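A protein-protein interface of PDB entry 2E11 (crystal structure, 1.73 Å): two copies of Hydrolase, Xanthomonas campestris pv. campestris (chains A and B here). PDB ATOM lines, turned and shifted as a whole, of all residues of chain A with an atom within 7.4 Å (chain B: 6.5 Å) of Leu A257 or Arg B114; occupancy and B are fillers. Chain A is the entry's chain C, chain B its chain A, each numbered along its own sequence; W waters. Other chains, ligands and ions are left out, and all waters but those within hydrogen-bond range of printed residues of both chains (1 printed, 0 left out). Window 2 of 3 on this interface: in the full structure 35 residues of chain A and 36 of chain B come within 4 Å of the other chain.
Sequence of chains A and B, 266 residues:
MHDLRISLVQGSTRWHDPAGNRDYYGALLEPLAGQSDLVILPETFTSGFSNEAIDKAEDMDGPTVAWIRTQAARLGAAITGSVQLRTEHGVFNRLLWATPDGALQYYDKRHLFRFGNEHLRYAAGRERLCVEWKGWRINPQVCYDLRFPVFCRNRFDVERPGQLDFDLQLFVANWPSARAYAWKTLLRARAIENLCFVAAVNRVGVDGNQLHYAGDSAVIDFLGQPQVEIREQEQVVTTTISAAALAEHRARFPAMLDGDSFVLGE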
ATOM      1  N   PHE A 156      -5.598 -15.702  25.012  1.00  0.00           N
ATOM      2  CA  PHE A 156      -5.308 -15.661  26.441  1.00  0.00           C
ATOM      3  C   PHE A 156      -5.270 -14.212  26.930  1.00  0.00           C
ATOM      4  O   PHE A 156      -4.667 -13.345  26.277  1.00  0.00           O
ATOM      5  CB  PHE A 156      -3.968 -16.374  26.751  1.00  0.00           C
ATOM      6  CG  PHE A 156      -3.610 -16.380  28.217  1.00  0.00           C
ATOM      7  CD1 PHE A 156      -2.647 -15.510  28.714  1.00  0.00           C
ATOM      8  CD2 PHE A 156      -4.245 -17.254  29.099  1.00  0.00           C
ATOM      9  CE1 PHE A 156      -2.337 -15.500  30.055  1.00  0.00           C
ATOM     10  CE2 PHE A 156      -3.935 -17.256  30.435  1.00  0.00           C
ATOM     11  CZ  PHE A 156      -2.989 -16.377  30.922  1.00  0.00           C
ATOM     12  N   GLY A 162      -6.276 -13.137  32.581  1.00  0.00           N
ATOM     13  CA  GLY A 162      -5.388 -14.233  32.948  1.00  0.00           C
ATOM     14  C   GLY A 162      -5.960 -15.602  32.627  1.00  0.00           C
ATOM     15  O   GLY A 162      -5.541 -16.612  33.210  1.00  0.00           O
ATOM     16  N   LEU A 164      -7.930 -18.171  29.264  1.00  0.00           N
ATOM     17  CA  LEU A 164      -8.356 -18.294  27.856  1.00  0.00           C
ATOM     18  C   LEU A 164      -9.769 -17.713  27.655  1.00  0.00           C
ATOM     19  O   LEU A 164     -10.557 -17.660  28.607  1.00  0.00           O
ATOM     20  CB  LEU A 164      -8.327 -19.754  27.412  1.00  0.00           C
ATOM     21  CG  LEU A 164      -6.920 -20.343  27.235  1.00  0.00           C
ATOM     22  CD1 LEU A 164      -6.915 -21.890  27.312  1.00  0.00           C
ATOM     23  CD2 LEU A 164      -6.273 -19.860  25.948  1.00  0.00           C
ATOM     24  N   LEU A 195      -6.773 -25.659  23.534  1.00  0.00           N
ATOM     25  CA  LEU A 195      -6.754 -26.205  24.883  1.00  0.00           C
ATOM     26  C   LEU A 195      -8.164 -26.219  25.484  1.00  0.00           C
ATOM     27  O   LEU A 195      -8.396 -25.698  26.567  1.00  0.00           O
ATOM     28  CB  LEU A 195      -5.841 -25.361  25.782  1.00  0.00           C
ATOM     29  CG  LEU A 195      -4.331 -25.261  25.558  1.00  0.00           C
ATOM     30  CD1 LEU A 195      -3.720 -26.592  25.248  1.00  0.00           C
ATOM     31  CD2 LEU A 195      -3.981 -24.262  24.499  1.00  0.00           C
ATOM     32  N   ARG A 250      -4.670 -27.294  31.600  1.00  0.00           N
ATOM     33  CA  ARG A 250      -4.226 -25.919  31.366  1.00  0.00           C
ATOM     34  C   ARG A 250      -3.111 -25.534  32.340  1.00  0.00           C
ATOM     35  O   ARG A 250      -2.210 -24.766  31.999  1.00  0.00           O
ATOM     36  CB  ARG A 250      -5.420 -24.969  31.472  1.00  0.00           C
ATOM     37  CG  ARG A 250      -6.375 -25.175  30.274  1.00  0.00           C
ATOM     38  CD  ARG A 250      -7.597 -24.318  30.379  1.00  0.00           C
ATOM     39  NE  ARG A 250      -8.353 -24.347  29.127  1.00  0.00           N
ATOM     40  CZ  ARG A 250      -9.478 -23.685  28.918  1.00  0.00           C
ATOM     41  NH1 ARG A 250     -10.014 -22.961  29.897  1.00  0.00           N
ATOM     42  NH2 ARG A 250     -10.088 -23.778  27.736  1.00  0.00           N
ATOM     43  N   PHE A 253       0.063 -27.960  31.033  1.00  0.00           N
ATOM     44  CA  PHE A 253       0.611 -27.677  29.713  1.00  0.00           C
ATOM     45  C   PHE A 253       0.251 -26.239  29.344  1.00  0.00           C
ATOM     46  O   PHE A 253      -0.824 -25.991  28.781  1.00  0.00           O
ATOM     47  CB  PHE A 253       0.061 -28.670  28.686  1.00  0.00           C
ATOM     48  CG  PHE A 253       0.812 -28.677  27.397  1.00  0.00           C
ATOM     49  CD1 PHE A 253       2.073 -29.289  27.312  1.00  0.00           C
ATOM     50  CD2 PHE A 253       0.263 -28.090  26.255  1.00  0.00           C
ATOM     51  CE1 PHE A 253       2.788 -29.304  26.098  1.00  0.00           C
ATOM     52  CE2 PHE A 253       0.968 -28.079  25.046  1.00  0.00           C
ATOM     53  CZ  PHE A 253       2.235 -28.691  24.969  1.00  0.00           C
ATOM     54  N   PRO A 254       1.153 -25.290  29.676  1.00  0.00           N
ATOM     55  CA  PRO A 254       0.825 -23.864  29.717  1.00  0.00           C
ATOM     56  C   PRO A 254       0.955 -23.156  28.372  1.00  0.00           C
ATOM     57  O   PRO A 254       1.444 -22.023  28.313  1.00  0.00           O
ATOM     58  CB  PRO A 254       1.856 -23.315  30.728  1.00  0.00           C
ATOM     59  CG  PRO A 254       3.055 -24.149  30.509  1.00  0.00           C
ATOM     60  CD  PRO A 254       2.566 -25.532  30.063  1.00  0.00           C
ATOM     61  N   ALA A 255       0.473 -23.809  27.311  1.00  0.00           N
ATOM     62  CA  ALA A 255       0.633 -23.294  25.966  1.00  0.00           C
ATOM     63  C   ALA A 255      -0.137 -21.992  25.784  1.00  0.00           C
ATOM     64  O   ALA A 255       0.196 -21.217  24.893  1.00  0.00           O
ATOM     65  CB  ALA A 255       0.207 -24.328  24.929  1.00  0.00           C
ATOM     66  N   MET A 256      -1.146 -21.769  26.636  1.00  0.00           N
ATOM     67  CA  MET A 256      -1.925 -20.518  26.601  1.00  0.00           C
ATOM     68  C   MET A 256      -1.023 -19.301  26.746  1.00  0.00           C
ATOM     69  O   MET A 256      -1.295 -18.240  26.196  1.00  0.00           O
ATOM     70  CB  MET A 256      -3.038 -20.519  27.665  1.00  0.00           C
ATOM     71  CG  MET A 256      -2.585 -20.782  29.138  1.00  0.00           C
ATOM     72  SD  MET A 256      -4.047 -21.029  30.230  1.00  0.00           S
ATOM     73  CE  MET A 256      -3.173 -21.344  31.771  1.00  0.00           C
ATOM     74  N   LEU A 257       0.077 -19.467  27.480  1.00  0.00           N
ATOM     75  CA  LEU A 257       0.973 -18.343  27.762  1.00  0.00           C
ATOM     76  C   LEU A 257       1.820 -17.933  26.575  1.00  0.00           C
ATOM     77  O   LEU A 257       2.436 -16.863  26.589  1.00  0.00           O
ATOM     78  CB  LEU A 257       1.884 -18.663  28.947  1.00  0.00           C
ATOM     79  CG  LEU A 257       1.186 -19.013  30.250  1.00  0.00           C
ATOM     80  CD1 LEU A 257       2.204 -19.431  31.308  1.00  0.00           C
ATOM     81  CD2 LEU A 257       0.304 -17.839  30.745  1.00  0.00           C
ATOM     82  N   ASP A 258       1.875 -18.797  25.569  1.00  0.00           N
ATOM     83  CA  ASP A 258       2.701 -18.550  24.396  1.00  0.00           C
ATOM     84  C   ASP A 258       1.960 -18.056  23.150  1.00  0.00           C
ATOM     85  O   ASP A 258       2.604 -17.723  22.142  1.00  0.00           O
ATOM     86  CB  ASP A 258       3.509 -19.811  24.097  1.00  0.00           C
ATOM     87  CG  ASP A 258       4.466 -20.146  25.218  1.00  0.00           C
ATOM     88  OD1 ASP A 258       5.186 -19.205  25.642  1.00  0.00           O
ATOM     89  OD2 ASP A 258       4.493 -21.310  25.683  1.00  0.00           O
ATOM     90  N   GLY A 259       0.628 -18.010  23.199  1.00  0.00           N
ATOM     91  CA  GLY A 259      -0.153 -17.536  22.045  1.00  0.00           C
ATOM     92  C   GLY A 259       0.174 -16.100  21.665  1.00  0.00           C
ATOM     93  O   GLY A 259       0.582 -15.269  22.512  1.00  0.00           O
ATOM     94  N   ASP A 260      -0.009 -15.795  20.390  1.00  0.00           N
ATOM     95  CA  ASP A 260       0.344 -14.485  19.840  1.00  0.00           C
ATOM     96  C   ASP A 260      -0.810 -13.508  19.912  1.00  0.00           C
ATOM     97  O   ASP A 260      -1.958 -13.886  19.701  1.00  0.00           O
ATOM     98  CB  ASP A 260       0.777 -14.639  18.382  1.00  0.00           C
ATOM     99  CG  ASP A 260       2.000 -15.513  18.246  1.00  0.00           C
ATOM    100  OD1 ASP A 260       3.088 -15.075  18.698  1.00  0.00           O
ATOM    101  OD2 ASP A 260       1.860 -16.647  17.741  1.00  0.00           O
ATOM    102  N   HIS B 111       8.237 -19.407  19.053  1.00  0.00           N
ATOM    103  CA  HIS B 111       7.577 -19.935  20.255  1.00  0.00           C
ATOM    104  C   HIS B 111       8.538 -20.907  20.898  1.00  0.00           C
ATOM    105  O   HIS B 111       8.663 -22.044  20.432  1.00  0.00           O
ATOM    106  CB  HIS B 111       6.287 -20.666  19.872  1.00  0.00           C
ATOM    107  CG  HIS B 111       5.346 -19.824  19.076  1.00  0.00           C
ATOM    108  ND1 HIS B 111       5.356 -19.807  17.698  1.00  0.00           N
ATOM    109  CD2 HIS B 111       4.401 -18.932  19.462  1.00  0.00           C
ATOM    110  CE1 HIS B 111       4.437 -18.957  17.269  1.00  0.00           C
ATOM    111  NE2 HIS B 111       3.853 -18.404  18.319  1.00  0.00           N
ATOM    112  N   LEU B 112       9.267 -20.454  21.927  1.00  0.00           N
ATOM    113  CA  LEU B 112      10.177 -21.382  22.601  1.00  0.00           C
ATOM    114  C   LEU B 112       9.356 -22.345  23.432  1.00  0.00           C
ATOM    115  O   LEU B 112       8.330 -21.988  23.980  1.00  0.00           O
ATOM    116  CB  LEU B 112      11.221 -20.662  23.474  1.00  0.00           C
ATOM    117  CG  LEU B 112      12.152 -19.714  22.698  1.00  0.00           C
ATOM    118  CD1 LEU B 112      13.076 -18.959  23.636  1.00  0.00           C
ATOM    119  CD2 LEU B 112      12.951 -20.489  21.639  1.00  0.00           C
ATOM    120  N   PHE B 113       9.827 -23.569  23.526  1.00  0.00           N
ATOM    121  CA  PHE B 113       9.029 -24.627  24.127  1.00  0.00           C
ATOM    122  C   PHE B 113       9.049 -24.534  25.663  1.00  0.00           C
ATOM    123  O   PHE B 113       9.926 -25.088  26.326  1.00  0.00           O
ATOM    124  CB  PHE B 113       9.504 -25.994  23.632  1.00  0.00           C
ATOM    125  CG  PHE B 113       8.660 -27.140  24.101  1.00  0.00           C
ATOM    126  CD1 PHE B 113       7.257 -27.112  23.959  1.00  0.00           C
ATOM    127  CD2 PHE B 113       9.260 -28.281  24.634  1.00  0.00           C
ATOM    128  CE1 PHE B 113       6.472 -28.192  24.363  1.00  0.00           C
ATOM    129  CE2 PHE B 113       8.471 -29.376  25.038  1.00  0.00           C
ATOM    130  CZ  PHE B 113       7.082 -29.331  24.895  1.00  0.00           C
ATOM    131  N   ARG B 114       8.060 -23.819  26.191  1.00  0.00           N
ATOM    132  CA  ARG B 114       7.909 -23.576  27.619  1.00  0.00           C
ATOM    133  C   ARG B 114       7.878 -24.856  28.456  1.00  0.00           C
ATOM    134  O   ARG B 114       8.513 -24.939  29.515  1.00  0.00           O
ATOM    135  CB  ARG B 114       6.621 -22.783  27.846  1.00  0.00           C
ATOM    136  CG  ARG B 114       6.347 -22.396  29.268  1.00  0.00           C
ATOM    137  CD  ARG B 114       5.253 -21.313  29.315  1.00  0.00           C
ATOM    138  NE  ARG B 114       5.710 -20.245  30.208  1.00  0.00           N
ATOM    139  CZ  ARG B 114       5.903 -18.985  29.841  1.00  0.00           C
ATOM    140  NH1 ARG B 114       5.643 -18.585  28.596  1.00  0.00           N
ATOM    141  NH2 ARG B 114       6.343 -18.121  30.736  1.00  0.00           N
ATOM    142  N   PHE B 115       7.150 -25.863  27.980  1.00  0.00           N
ATOM    143  CA  PHE B 115       7.055 -27.118  28.727  1.00  0.00           C
ATOM    144  C   PHE B 115       8.411 -27.807  28.952  1.00  0.00           C
ATOM    145  O   PHE B 115       8.588 -28.510  29.968  1.00  0.00           O
ATOM    146  CB  PHE B 115       6.092 -28.062  28.027  1.00  0.00           C
ATOM    147  CG  PHE B 115       5.774 -29.302  28.813  1.00  0.00           C
ATOM    148  CD1 PHE B 115       4.803 -29.275  29.805  1.00  0.00           C
ATOM    149  CD2 PHE B 115       6.432 -30.497  28.546  1.00  0.00           C
ATOM    150  CE1 PHE B 115       4.486 -30.431  30.527  1.00  0.00           C
ATOM    151  CE2 PHE B 115       6.121 -31.662  29.267  1.00  0.00           C
ATOM    152  CZ  PHE B 115       5.147 -31.618  30.259  1.00  0.00           C
ATOM    153  N   GLY B 116       9.343 -27.614  28.017  1.00  0.00           N
ATOM    154  CA  GLY B 116      10.686 -28.196  28.103  1.00  0.00           C
ATOM    155  C   GLY B 116      11.722 -27.203  28.613  1.00  0.00           C
ATOM    156  O   GLY B 116      12.942 -27.428  28.489  1.00  0.00           O
ATOM    157  N   ASN B 117      11.225 -26.089  29.163  1.00  0.00           N
ATOM    158  CA  ASN B 117      12.069 -25.007  29.705  1.00  0.00           C
ATOM    159  C   ASN B 117      13.029 -24.335  28.732  1.00  0.00           C
ATOM    160  O   ASN B 117      14.017 -23.707  29.131  1.00  0.00           O
ATOM    161  CB  ASN B 117      12.775 -25.468  30.971  1.00  0.00           C
ATOM    162  CG  ASN B 117      11.796 -25.611  32.122  1.00  0.00           C
ATOM    163  OD1 ASN B 117      11.009 -24.699  32.373  1.00  0.00           O
ATOM    164  ND2 ASN B 117      11.790 -26.766  32.767  1.00  0.00           N
ATOM    165  N   GLU B 118      12.703 -24.432  27.447  1.00  0.00           N
ATOM    166  CA  GLU B 118      13.493 -23.779  26.418  1.00  0.00           C
ATOM    167  C   GLU B 118      13.476 -22.251  26.578  1.00  0.00           C
ATOM    168  O   GLU B 118      14.416 -21.583  26.202  1.00  0.00           O
ATOM    169  CB  GLU B 118      12.997 -24.191  25.025  1.00  0.00           C
ATOM    170  CG  GLU B 118      13.945 -23.743  23.891  1.00  0.00           C
ATOM    171  CD  GLU B 118      13.451 -24.064  22.489  1.00  0.00           C
ATOM    172  OE1 GLU B 118      14.290 -24.014  21.563  1.00  0.00           O
ATOM    173  OE2 GLU B 118      12.251 -24.349  22.308  1.00  0.00           O
ATOM    174  N   HIS B 119      12.413 -21.717  27.162  1.00  0.00           N
ATOM    175  CA  HIS B 119      12.220 -20.259  27.273  1.00  0.00           C
ATOM    176  C   HIS B 119      13.078 -19.604  28.370  1.00  0.00           C
ATOM    177  O   HIS B 119      13.187 -18.380  28.437  1.00  0.00           O
ATOM    178  CB  HIS B 119      10.746 -19.991  27.575  1.00  0.00           C
ATOM    179  CG  HIS B 119      10.293 -20.612  28.858  1.00  0.00           C
ATOM    180  ND1 HIS B 119       9.695 -19.893  29.872  1.00  0.00           N
ATOM    181  CD2 HIS B 119      10.410 -21.876  29.314  1.00  0.00           C
ATOM    182  CE1 HIS B 119       9.438 -20.697  30.890  1.00  0.00           C
ATOM    183  NE2 HIS B 119       9.868 -21.906  30.580  1.00  0.00           N
ATOM    184  N   TYR B 144       7.470 -26.532  18.260  1.00  0.00           N
ATOM    185  CA  TYR B 144       6.362 -25.941  19.045  1.00  0.00           C
ATOM    186  C   TYR B 144       5.562 -24.925  18.253  1.00  0.00           C
ATOM    187  O   TYR B 144       4.369 -24.711  18.531  1.00  0.00           O
ATOM    188  CB  TYR B 144       6.953 -25.277  20.276  1.00  0.00           C
ATOM    189  CG  TYR B 144       6.021 -24.847  21.396  1.00  0.00           C
ATOM    190  CD1 TYR B 144       6.230 -23.621  22.024  1.00  0.00           C
ATOM    191  CD2 TYR B 144       4.994 -25.673  21.877  1.00  0.00           C
ATOM    192  CE1 TYR B 144       5.436 -23.196  23.084  1.00  0.00           C
ATOM    193  CE2 TYR B 144       4.184 -25.257  22.956  1.00  0.00           C
ATOM    194  CZ  TYR B 144       4.416 -24.013  23.540  1.00  0.00           C
ATOM    195  OH  TYR B 144       3.655 -23.599  24.596  1.00  0.00           O
ATOM    196  N   PHE B 148       0.544 -23.062  17.008  1.00  0.00           N
ATOM    197  CA  PHE B 148       0.135 -21.646  16.955  1.00  0.00           C
ATOM    198  C   PHE B 148      -0.383 -21.262  15.591  1.00  0.00           C
ATOM    199  O   PHE B 148       0.376 -20.802  14.737  1.00  0.00           O
ATOM    200  CB  PHE B 148       1.260 -20.729  17.447  1.00  0.00           C
ATOM    201  CG  PHE B 148       1.667 -21.057  18.829  1.00  0.00           C
ATOM    202  CD1 PHE B 148       2.673 -21.993  19.053  1.00  0.00           C
ATOM    203  CD2 PHE B 148       0.955 -20.536  19.923  1.00  0.00           C
ATOM    204  CE1 PHE B 148       3.010 -22.371  20.344  1.00  0.00           C
ATOM    205  CE2 PHE B 148       1.293 -20.908  21.219  1.00  0.00           C
ATOM    206  CZ  PHE B 148       2.314 -21.832  21.424  1.00  0.00           C
HETATM  207  O   HOH W   1       7.801 -19.987  25.723  1.00  0.00           O
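The guanidinium group (NH1) of Arg B114 is in salt-bridge range of the side-chain carboxylate (OD1) of Asp A258 (3.1 Å).
The side-chain hydroxyl of Tyr B144 lies within hydrogen-bond range of the side-chain carboxylate of Asp A258 (2.7 Å).
A ring nitrogen (NE2) of His B111 lies within hydrogen-bond range of the side-chain carboxylate of Asp A260 (2.7 Å).
A ring nitrogen (NE2) of His B119 sits at hydrogen-bond distance from the backbone carbonyl oxygen (O) of Arg B114, 3.5 Å away.
Phe B115 touches Phe A253.
CD of Arg B114 touches CG of Pro A254, at 3.8 Å.
Tyr B144 touches Ala A255 (OH to CA, 3.3 Å).
CE2 of Phe B148 touches O of Ala A255, at 3.8 Å.
Arg B114 touches Leu A257 (NE to CD1, 3.8 Å).
Asp A258 touches His B111 (O to CD2, 3.4 Å).
CE2 of Phe B148 touches C of Asp A258 (3.5 Å).
Gly A259 touches Phe B148 (N to CE2, 3.6 Å).
Of the printed residues of chain B, Ala A255 touches Tyr B144 and Phe B148.
Leu A257 touches just one residue of chain B: Arg B114 (3.8 Å).
Printed residues of chain B within 4 Å of Asp A260: His B111 (2.7 Å).
Of the printed residues of chain A, Arg B114 touches Pro A254, Leu A257 and Asp A258.
Printed residues of chain A within 4 Å of Phe B115: Phe A253 (3.7 Å).
Glu B118 touches none of the printed residues of chain A.
The nearest residue of chain A that does not touch Arg B114 is Ala A255 (5.8 Å).
Of the 11 printed residues of chain B, 5 touch a printed residue of chain A.
Among the printed residues, 11 pairs touch across the chains.
Among the printed residues, Asp or Glu carboxylates within 4 Å of a Lys or Arg side-chain nitrogen of the other chain: Asp A258 with Arg B114 (3.1 Å).
No position is printed for both chains.
Of the 11 pairs that touch across the chains among the printed residues, none has its exchanged pair printed and touching as well.
Water W1 lies within hydrogen-bond range of O of Leu B112 (2.7 Å) and OD1 of Asp A258 (2.7 Å).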
